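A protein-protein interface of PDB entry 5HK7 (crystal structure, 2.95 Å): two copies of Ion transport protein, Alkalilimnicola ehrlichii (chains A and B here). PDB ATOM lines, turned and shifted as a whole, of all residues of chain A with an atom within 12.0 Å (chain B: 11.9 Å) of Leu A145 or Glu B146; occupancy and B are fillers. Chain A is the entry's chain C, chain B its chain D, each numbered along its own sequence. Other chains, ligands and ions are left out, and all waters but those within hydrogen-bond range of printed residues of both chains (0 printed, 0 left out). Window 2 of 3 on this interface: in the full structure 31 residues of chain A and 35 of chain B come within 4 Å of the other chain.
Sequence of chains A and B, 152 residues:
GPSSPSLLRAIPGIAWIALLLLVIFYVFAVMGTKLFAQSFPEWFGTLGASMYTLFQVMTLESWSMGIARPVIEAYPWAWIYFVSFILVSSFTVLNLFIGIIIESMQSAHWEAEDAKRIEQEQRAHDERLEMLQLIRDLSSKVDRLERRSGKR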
ATOM      1  N   LEU A 134      23.006  40.981  32.724  1.00  0.00           N
ATOM      2  CA  LEU A 134      23.357  39.930  31.769  1.00  0.00           C
ATOM      3  C   LEU A 134      24.430  39.125  32.407  1.00  0.00           C
ATOM      4  O   LEU A 134      24.324  37.919  32.405  1.00  0.00           O
ATOM      5  CB  LEU A 134      23.839  40.440  30.435  1.00  0.00           C
ATOM      6  CG  LEU A 134      22.996  41.578  29.928  1.00  0.00           C
ATOM      7  CD1 LEU A 134      23.254  41.715  28.466  1.00  0.00           C
ATOM      8  CD2 LEU A 134      21.543  41.267  30.128  1.00  0.00           C
ATOM      9  N   ARG A 136      25.221  38.578  35.351  1.00  0.00           N
ATOM     10  CA  ARG A 136      24.786  37.702  36.404  1.00  0.00           C
ATOM     11  C   ARG A 136      24.088  36.478  35.853  1.00  0.00           C
ATOM     12  O   ARG A 136      24.230  35.393  36.391  1.00  0.00           O
ATOM     13  CB  ARG A 136      23.897  38.439  37.370  1.00  0.00           C
ATOM     14  CG  ARG A 136      24.733  38.887  38.526  1.00  0.00           C
ATOM     15  CD  ARG A 136      23.929  39.019  39.784  1.00  0.00           C
ATOM     16  NE  ARG A 136      24.561  40.057  40.581  1.00  0.00           N
ATOM     17  CZ  ARG A 136      24.212  41.343  40.559  1.00  0.00           C
ATOM     18  NH1 ARG A 136      23.204  41.771  39.791  1.00  0.00           N
ATOM     19  NH2 ARG A 136      24.876  42.197  41.328  1.00  0.00           N
ATOM     20  N   ASP A 137      23.357  36.673  34.770  1.00  0.00           N
ATOM     21  CA  ASP A 137      22.684  35.611  34.055  1.00  0.00           C
ATOM     22  C   ASP A 137      23.591  34.679  33.307  1.00  0.00           C
ATOM     23  O   ASP A 137      23.306  33.515  33.175  1.00  0.00           O
ATOM     24  CB  ASP A 137      21.723  36.225  33.049  1.00  0.00           C
ATOM     25  CG  ASP A 137      20.558  36.908  33.729  1.00  0.00           C
ATOM     26  OD1 ASP A 137      20.301  36.576  34.922  1.00  0.00           O
ATOM     27  OD2 ASP A 137      19.904  37.774  33.092  1.00  0.00           O
ATOM     28  N   LEU A 138      24.655  35.219  32.757  1.00  0.00           N
ATOM     29  CA  LEU A 138      25.620  34.459  32.023  1.00  0.00           C
ATOM     30  C   LEU A 138      26.388  33.653  33.018  1.00  0.00           C
ATOM     31  O   LEU A 138      26.820  32.563  32.728  1.00  0.00           O
ATOM     32  CB  LEU A 138      26.555  35.436  31.386  1.00  0.00           C
ATOM     33  CG  LEU A 138      27.585  34.891  30.472  1.00  0.00           C
ATOM     34  CD1 LEU A 138      26.829  34.070  29.470  1.00  0.00           C
ATOM     35  CD2 LEU A 138      28.283  36.052  29.808  1.00  0.00           C
ATOM     36  N   SER A 139      26.572  34.199  34.204  1.00  0.00           N
ATOM     37  CA  SER A 139      27.185  33.430  35.248  1.00  0.00           C
ATOM     38  C   SER A 139      26.297  32.269  35.682  1.00  0.00           C
ATOM     39  O   SER A 139      26.776  31.291  36.221  1.00  0.00           O
ATOM     40  CB  SER A 139      27.557  34.316  36.417  1.00  0.00           C
ATOM     41  OG  SER A 139      28.967  34.280  36.558  1.00  0.00           O
ATOM     42  N   SER A 140      25.005  32.358  35.414  1.00  0.00           N
ATOM     43  CA  SER A 140      24.113  31.240  35.691  1.00  0.00           C
ATOM     44  C   SER A 140      24.241  30.184  34.650  1.00  0.00           C
ATOM     45  O   SER A 140      24.348  29.020  34.954  1.00  0.00           O
ATOM     46  CB  SER A 140      22.665  31.686  35.683  1.00  0.00           C
ATOM     47  OG  SER A 140      22.286  32.067  36.976  1.00  0.00           O
ATOM     48  N   LYS A 141      24.177  30.596  33.401  1.00  0.00           N
ATOM     49  CA  LYS A 141      24.276  29.653  32.322  1.00  0.00           C
ATOM     50  C   LYS A 141      25.568  28.862  32.439  1.00  0.00           C
ATOM     51  O   LYS A 141      25.586  27.661  32.166  1.00  0.00           O
ATOM     52  CB  LYS A 141      24.218  30.362  30.977  1.00  0.00           C
ATOM     53  CG  LYS A 141      22.856  30.321  30.337  1.00  0.00           C
ATOM     54  CD  LYS A 141      22.813  31.206  29.115  1.00  0.00           C
ATOM     55  CE  LYS A 141      22.496  32.645  29.489  1.00  0.00           C
ATOM     56  NZ  LYS A 141      21.121  32.976  29.033  1.00  0.00           N
ATOM     57  N   VAL A 142      26.650  29.534  32.828  1.00  0.00           N
ATOM     58  CA  VAL A 142      27.944  28.901  32.844  1.00  0.00           C
ATOM     59  C   VAL A 142      27.935  28.073  34.066  1.00  0.00           C
ATOM     60  O   VAL A 142      28.560  27.051  34.103  1.00  0.00           O
ATOM     61  CB  VAL A 142      29.089  29.919  32.883  1.00  0.00           C
ATOM     62  CG1 VAL A 142      30.401  29.285  33.359  1.00  0.00           C
ATOM     63  CG2 VAL A 142      29.260  30.515  31.491  1.00  0.00           C
ATOM     64  N   ASP A 143      27.177  28.498  35.058  1.00  0.00           N
ATOM     65  CA  ASP A 143      27.041  27.703  36.279  1.00  0.00           C
ATOM     66  C   ASP A 143      26.271  26.426  36.103  1.00  0.00           C
ATOM     67  O   ASP A 143      26.537  25.452  36.785  1.00  0.00           O
ATOM     68  CB  ASP A 143      26.430  28.522  37.396  1.00  0.00           C
ATOM     69  CG  ASP A 143      27.493  28.999  38.377  1.00  0.00           C
ATOM     70  OD1 ASP A 143      28.643  28.482  38.310  1.00  0.00           O
ATOM     71  OD2 ASP A 143      27.196  29.894  39.197  1.00  0.00           O
ATOM     72  N   ARG A 144      25.337  26.433  35.163  1.00  0.00           N
ATOM     73  CA  ARG A 144      24.661  25.231  34.744  1.00  0.00           C
ATOM     74  C   ARG A 144      25.524  24.327  33.925  1.00  0.00           C
ATOM     75  O   ARG A 144      25.564  23.159  34.221  1.00  0.00           O
ATOM     76  CB  ARG A 144      23.402  25.556  33.981  1.00  0.00           C
ATOM     77  CG  ARG A 144      22.197  25.314  34.856  1.00  0.00           C
ATOM     78  CD  ARG A 144      21.181  26.448  34.802  1.00  0.00           C
ATOM     79  NE  ARG A 144      20.896  26.834  33.423  1.00  0.00           N
ATOM     80  CZ  ARG A 144      20.533  28.057  33.062  1.00  0.00           C
ATOM     81  NH1 ARG A 144      20.392  28.994  33.987  1.00  0.00           N
ATOM     82  NH2 ARG A 144      20.309  28.340  31.783  1.00  0.00           N
ATOM     83  N   LEU A 145      26.193  24.836  32.893  1.00  0.00           N
ATOM     84  CA  LEU A 145      27.129  24.019  32.144  1.00  0.00           C
ATOM     85  C   LEU A 145      28.043  23.256  33.052  1.00  0.00           C
ATOM     86  O   LEU A 145      28.474  22.162  32.682  1.00  0.00           O
ATOM     87  CB  LEU A 145      27.999  24.859  31.266  1.00  0.00           C
ATOM     88  CG  LEU A 145      27.339  25.293  29.977  1.00  0.00           C
ATOM     89  CD1 LEU A 145      28.407  25.826  29.026  1.00  0.00           C
ATOM     90  CD2 LEU A 145      26.613  24.164  29.264  1.00  0.00           C
ATOM     91  N   GLU A 146      28.349  23.813  34.226  1.00  0.00           N
ATOM     92  CA  GLU A 146      29.318  23.178  35.097  1.00  0.00           C
ATOM     93  C   GLU A 146      28.753  22.020  35.859  1.00  0.00           C
ATOM     94  O   GLU A 146      29.354  20.948  35.887  1.00  0.00           O
ATOM     95  CB  GLU A 146      29.963  24.151  36.053  1.00  0.00           C
ATOM     96  CG  GLU A 146      31.475  24.175  35.880  1.00  0.00           C
ATOM     97  CD  GLU A 146      32.159  25.133  36.836  1.00  0.00           C
ATOM     98  OE1 GLU A 146      31.750  26.320  36.881  1.00  0.00           O
ATOM     99  OE2 GLU A 146      33.097  24.696  37.543  1.00  0.00           O
ATOM    100  N   ARG A 147      27.600  22.228  36.476  1.00  0.00           N
ATOM    101  CA  ARG A 147      26.896  21.136  37.129  1.00  0.00           C
ATOM    102  C   ARG A 147      26.355  20.109  36.120  1.00  0.00           C
ATOM    103  O   ARG A 147      26.491  18.903  36.349  1.00  0.00           O
ATOM    104  CB  ARG A 147      25.757  21.658  37.992  1.00  0.00           C
ATOM    105  CG  ARG A 147      26.168  22.280  39.309  1.00  0.00           C
ATOM    106  CD  ARG A 147      24.928  22.630  40.134  1.00  0.00           C
ATOM    107  NE  ARG A 147      24.499  24.022  39.929  1.00  0.00           N
ATOM    108  CZ  ARG A 147      23.505  24.426  39.126  1.00  0.00           C
ATOM    109  NH1 ARG A 147      22.800  23.557  38.416  1.00  0.00           N
ATOM    110  NH2 ARG A 147      23.219  25.719  39.021  1.00  0.00           N
ATOM    111  N   ARG A 148      25.736  20.580  35.025  1.00  0.00           N
ATOM    112  CA  ARG A 148      25.209  19.663  33.993  1.00  0.00           C
ATOM    113  C   ARG A 148      26.409  18.833  33.549  1.00  0.00           C
ATOM    114  O   ARG A 148      26.239  17.678  33.179  1.00  0.00           O
ATOM    115  CB  ARG A 148      24.461  20.362  32.824  1.00  0.00           C
ATOM    116  N   SER A 149      27.611  19.401  33.735  1.00  0.00           N
ATOM    117  CA  SER A 149      28.909  18.874  33.237  1.00  0.00           C
ATOM    118  C   SER A 149      28.883  18.258  31.847  1.00  0.00           C
ATOM    119  O   SER A 149      29.515  18.771  30.939  1.00  0.00           O
ATOM    120  CB  SER A 149      29.557  17.894  34.219  1.00  0.00           C
ATOM    121  OG  SER A 149      30.861  18.335  34.525  1.00  0.00           O
ATOM    122  N   ASP B 137      26.166  38.811  22.804  1.00  0.00           N
ATOM    123  CA  ASP B 137      26.646  37.799  21.874  1.00  0.00           C
ATOM    124  C   ASP B 137      27.205  36.609  22.609  1.00  0.00           C
ATOM    125  O   ASP B 137      26.861  35.491  22.322  1.00  0.00           O
ATOM    126  CB  ASP B 137      27.660  38.389  20.896  1.00  0.00           C
ATOM    127  CG  ASP B 137      27.025  39.447  20.006  1.00  0.00           C
ATOM    128  OD1 ASP B 137      25.784  39.407  19.856  1.00  0.00           O
ATOM    129  OD2 ASP B 137      27.734  40.323  19.471  1.00  0.00           O
ATOM    130  N   LEU B 138      28.045  36.867  23.589  1.00  0.00           N
ATOM    131  CA  LEU B 138      28.607  35.828  24.411  1.00  0.00           C
ATOM    132  C   LEU B 138      27.505  35.014  25.056  1.00  0.00           C
ATOM    133  O   LEU B 138      27.625  33.810  25.178  1.00  0.00           O
ATOM    134  CB  LEU B 138      29.452  36.469  25.514  1.00  0.00           C
ATOM    135  CG  LEU B 138      30.119  35.460  26.401  1.00  0.00           C
ATOM    136  CD1 LEU B 138      31.184  34.864  25.541  1.00  0.00           C
ATOM    137  CD2 LEU B 138      30.806  36.030  27.587  1.00  0.00           C
ATOM    138  N   SER B 139      26.433  35.681  25.478  1.00  0.00           N
ATOM    139  CA  SER B 139      25.459  35.060  26.367  1.00  0.00           C
ATOM    140  C   SER B 139      24.700  34.009  25.621  1.00  0.00           C
ATOM    141  O   SER B 139      23.984  33.221  26.213  1.00  0.00           O
ATOM    142  CB  SER B 139      24.471  36.076  26.946  1.00  0.00           C
ATOM    143  OG  SER B 139      24.439  36.041  28.382  1.00  0.00           O
ATOM    144  N   SER B 140      24.864  34.011  24.312  1.00  0.00           N
ATOM    145  CA  SER B 140      24.056  33.183  23.466  1.00  0.00           C
ATOM    146  C   SER B 140      24.903  32.093  22.815  1.00  0.00           C
ATOM    147  O   SER B 140      24.363  31.162  22.245  1.00  0.00           O
ATOM    148  CB  SER B 140      23.410  34.048  22.399  1.00  0.00           C
ATOM    149  OG  SER B 140      24.390  34.329  21.411  1.00  0.00           O
ATOM    150  N   LYS B 141      26.222  32.223  22.865  1.00  0.00           N
ATOM    151  CA  LYS B 141      27.080  31.116  22.490  1.00  0.00           C
ATOM    152  C   LYS B 141      27.089  30.218  23.657  1.00  0.00           C
ATOM    153  O   LYS B 141      27.103  29.020  23.504  1.00  0.00           O
ATOM    154  CB  LYS B 141      28.514  31.528  22.256  1.00  0.00           C
ATOM    155  CG  LYS B 141      28.672  32.848  21.568  1.00  0.00           C
ATOM    156  CD  LYS B 141      30.149  33.112  21.394  1.00  0.00           C
ATOM    157  CE  LYS B 141      30.525  33.844  20.106  1.00  0.00           C
ATOM    158  NZ  LYS B 141      31.664  34.729  20.497  1.00  0.00           N
ATOM    159  N   VAL B 142      27.094  30.806  24.843  1.00  0.00           N
ATOM    160  CA  VAL B 142      27.186  30.030  26.043  1.00  0.00           C
ATOM    161  C   VAL B 142      25.940  29.248  26.163  1.00  0.00           C
ATOM    162  O   VAL B 142      25.887  28.350  26.982  1.00  0.00           O
ATOM    163  CB  VAL B 142      27.360  30.878  27.308  1.00  0.00           C
ATOM    164  CG1 VAL B 142      27.107  30.045  28.583  1.00  0.00           C
ATOM    165  CG2 VAL B 142      28.767  31.460  27.313  1.00  0.00           C
ATOM    166  N   ASP B 143      24.933  29.562  25.367  1.00  0.00           N
ATOM    167  CA  ASP B 143      23.776  28.722  25.479  1.00  0.00           C
ATOM    168  C   ASP B 143      23.385  28.042  24.198  1.00  0.00           C
ATOM    169  O   ASP B 143      22.384  27.360  24.140  1.00  0.00           O
ATOM    170  CB  ASP B 143      22.617  29.409  26.224  1.00  0.00           C
ATOM    171  CG  ASP B 143      21.866  30.366  25.382  1.00  0.00           C
ATOM    172  OD1 ASP B 143      22.152  30.416  24.154  1.00  0.00           O
ATOM    173  OD2 ASP B 143      20.989  31.050  25.980  1.00  0.00           O
ATOM    174  N   ARG B 144      24.208  28.176  23.179  1.00  0.00           N
ATOM    175  CA  ARG B 144      24.185  27.167  22.160  1.00  0.00           C
ATOM    176  C   ARG B 144      25.162  26.039  22.489  1.00  0.00           C
ATOM    177  O   ARG B 144      25.015  24.981  21.945  1.00  0.00           O
ATOM    178  CB  ARG B 144      24.352  27.762  20.759  1.00  0.00           C
ATOM    179  CG  ARG B 144      25.777  27.749  20.302  1.00  0.00           C
ATOM    180  CD  ARG B 144      25.917  27.990  18.810  1.00  0.00           C
ATOM    181  NE  ARG B 144      27.173  28.696  18.579  1.00  0.00           N
ATOM    182  CZ  ARG B 144      27.332  29.711  17.747  1.00  0.00           C
ATOM    183  NH1 ARG B 144      26.305  30.137  17.003  1.00  0.00           N
ATOM    184  NH2 ARG B 144      28.526  30.296  17.673  1.00  0.00           N
ATOM    185  N   LEU B 145      26.108  26.236  23.407  1.00  0.00           N
ATOM    186  CA  LEU B 145      26.754  25.098  24.089  1.00  0.00           C
ATOM    187  C   LEU B 145      25.734  24.358  24.909  1.00  0.00           C
ATOM    188  O   LEU B 145      25.714  23.144  24.909  1.00  0.00           O
ATOM    189  CB  LEU B 145      27.810  25.518  25.085  1.00  0.00           C
ATOM    190  CG  LEU B 145      29.187  25.994  24.682  1.00  0.00           C
ATOM    191  CD1 LEU B 145      29.964  26.142  25.980  1.00  0.00           C
ATOM    192  CD2 LEU B 145      29.879  25.063  23.699  1.00  0.00           C
ATOM    193  N   GLU B 146      24.895  25.083  25.638  1.00  0.00           N
ATOM    194  CA  GLU B 146      23.941  24.436  26.513  1.00  0.00           C
ATOM    195  C   GLU B 146      22.989  23.578  25.724  1.00  0.00           C
ATOM    196  O   GLU B 146      22.346  22.689  26.283  1.00  0.00           O
ATOM    197  CB  GLU B 146      23.140  25.446  27.306  1.00  0.00           C
ATOM    198  CG  GLU B 146      23.408  25.374  28.800  1.00  0.00           C
ATOM    199  CD  GLU B 146      22.597  26.355  29.650  1.00  0.00           C
ATOM    200  OE1 GLU B 146      21.714  27.117  29.134  1.00  0.00           O
ATOM    201  OE2 GLU B 146      22.870  26.347  30.878  1.00  0.00           O
ATOM    202  N   ARG B 147      22.891  23.836  24.426  1.00  0.00           N
ATOM    203  CA  ARG B 147      22.015  23.038  23.586  1.00  0.00           C
ATOM    204  C   ARG B 147      22.735  22.096  22.648  1.00  0.00           C
ATOM    205  O   ARG B 147      22.199  21.058  22.315  1.00  0.00           O
ATOM    206  CB  ARG B 147      21.119  23.923  22.751  1.00  0.00           C
ATOM    207  CG  ARG B 147      21.702  24.199  21.371  1.00  0.00           C
ATOM    208  CD  ARG B 147      20.766  25.070  20.543  1.00  0.00           C
ATOM    209  NE  ARG B 147      19.914  25.917  21.393  1.00  0.00           N
ATOM    210  CZ  ARG B 147      19.878  27.253  21.376  1.00  0.00           C
ATOM    211  NH1 ARG B 147      20.642  27.948  20.539  1.00  0.00           N
ATOM    212  NH2 ARG B 147      19.070  27.900  22.209  1.00  0.00           N
ATOM    213  N   ARG B 148      23.908  22.479  22.169  1.00  0.00           N
ATOM    214  CA  ARG B 148      24.635  21.624  21.245  1.00  0.00           C
ATOM    215  C   ARG B 148      25.442  20.688  22.143  1.00  0.00           C
ATOM    216  O   ARG B 148      26.483  20.130  21.748  1.00  0.00           O
ATOM    217  CB  ARG B 148      25.516  22.441  20.283  1.00  0.00           C
ATOM    218  CG  ARG B 148      24.755  23.367  19.325  1.00  0.00           C
ATOM    219  CD  ARG B 148      25.520  23.630  18.021  1.00  0.00           C
ATOM    220  NE  ARG B 148      26.979  23.757  18.190  1.00  0.00           N
ATOM    221  CZ  ARG B 148      27.775  24.557  17.469  1.00  0.00           C
ATOM    222  NH1 ARG B 148      27.279  25.311  16.495  1.00  0.00           N
ATOM    223  NH2 ARG B 148      29.085  24.590  17.707  1.00  0.00           N
ATOM    224  N   SER B 149      24.943  20.574  23.380  1.00  0.00           N
ATOM    225  CA  SER B 149      25.296  19.533  24.333  1.00  0.00           C
ATOM    226  C   SER B 149      24.194  19.430  25.382  1.00  0.00           C
ATOM    227  O   SER B 149      23.644  18.358  25.629  1.00  0.00           O
ATOM    228  CB  SER B 149      26.614  19.860  25.033  1.00  0.00           C
ATOM    229  OG  SER B 149      26.912  18.825  25.932  1.00  0.00           O
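Hydrophobic or aromatic side chains of chain A that line the printed part of chain B: Leu A138, Val A142 and Leu A145.
Along chain A the printed residues that touch a printed residue of chain B span positions 138 to 145.
Of the 13 printed residues of chain B, 6 touch a printed residue of chain A.
Printed residues of chain B that touch a printed residue of chain A: Leu B138, Ser B139, Val B142, Asp B143, Leu B145 and Glu B146.
Among the printed residues, 11 pairs touch across the chains.
Among the printed residues, Asp or Glu carboxylates within 4 Å of a Lys or Arg side-chain nitrogen of the other chain: Lys A141 with Asp B143 and Arg A144 with Glu B146.
Among the printed residues, merely in contact across the chains: Leu A138 with Ser B139 (3.3 Å), Leu A138 with Leu B138 (3.4 Å), Leu A145 with Leu B145 (3.4 Å), Leu A145 with Glu B146 (3.5 Å), Lys A141 with Ser B139 (3.6 Å), Val A142 with Val B142 (3.6 Å), Lys A141 with Val B142 (3.8 Å) and Leu A138 with Val B142 (3.9 Å).
The side-chain amino group of Lys A141 lies within salt-bridge range of the side-chain carboxylate of Asp B143, at 3.6 Å.
OE1 of Glu B146 lies within salt-bridge range of NH2 of Arg A144, at 3.2 Å.
The backbone carbonyl oxygen of Lys A141 sits close to the side-chain carboxylate of Glu B146, 3.3 Å away.
Leu B138 touches its own counterpart, Leu A138.
Leu A138 touches Ser B139, but with the chains exchanged Ser A139 does not touch Leu B138 (8.1 Å).
Lys A141 touches Glu B146, but with the chains exchanged Glu A146 does not touch Lys B141 (12.0 Å).
Leu A145 touches Glu B146, but with the chains exchanged Glu A146 does not touch Leu B145 (8.7 Å).
13 positions are printed for both chains.
Leu A145 touches just these residues of chain B: Leu B145 and Glu B146.
Glu B146 touches three residues of chain A.
Of chain B, only Val B142 comes within 4 Å of Val A142.
No residue of chain B comes within 4 Å of Glu A146.
No residue of chain B comes within 4 Å of Arg A147.
No residue of chain B comes within 4 Å of Arg A148.
No residue of chain B comes within 4 Å of Ser A149.
Printed residues of chain A within 4 Å of Val B142: Leu A138, Lys A141 and Val A142.
No residue of chain A comes within 4 Å of Arg B147.
No residue of chain A comes within 4 Å of Ser B149.
Printed residues of chain B within 4 Å of Leu A138: Leu B138, Ser B139 and Val B142.
Of the printed residues of chain A, Ser B139 touches Leu A138 and Lys A141.
Of the printed residues of chain A, Leu B138 touches Leu A138 (3.4 Å).
Ser A139 touches none of the printed residues of chain B.
Ser A140 touches none of the printed residues of chain B.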
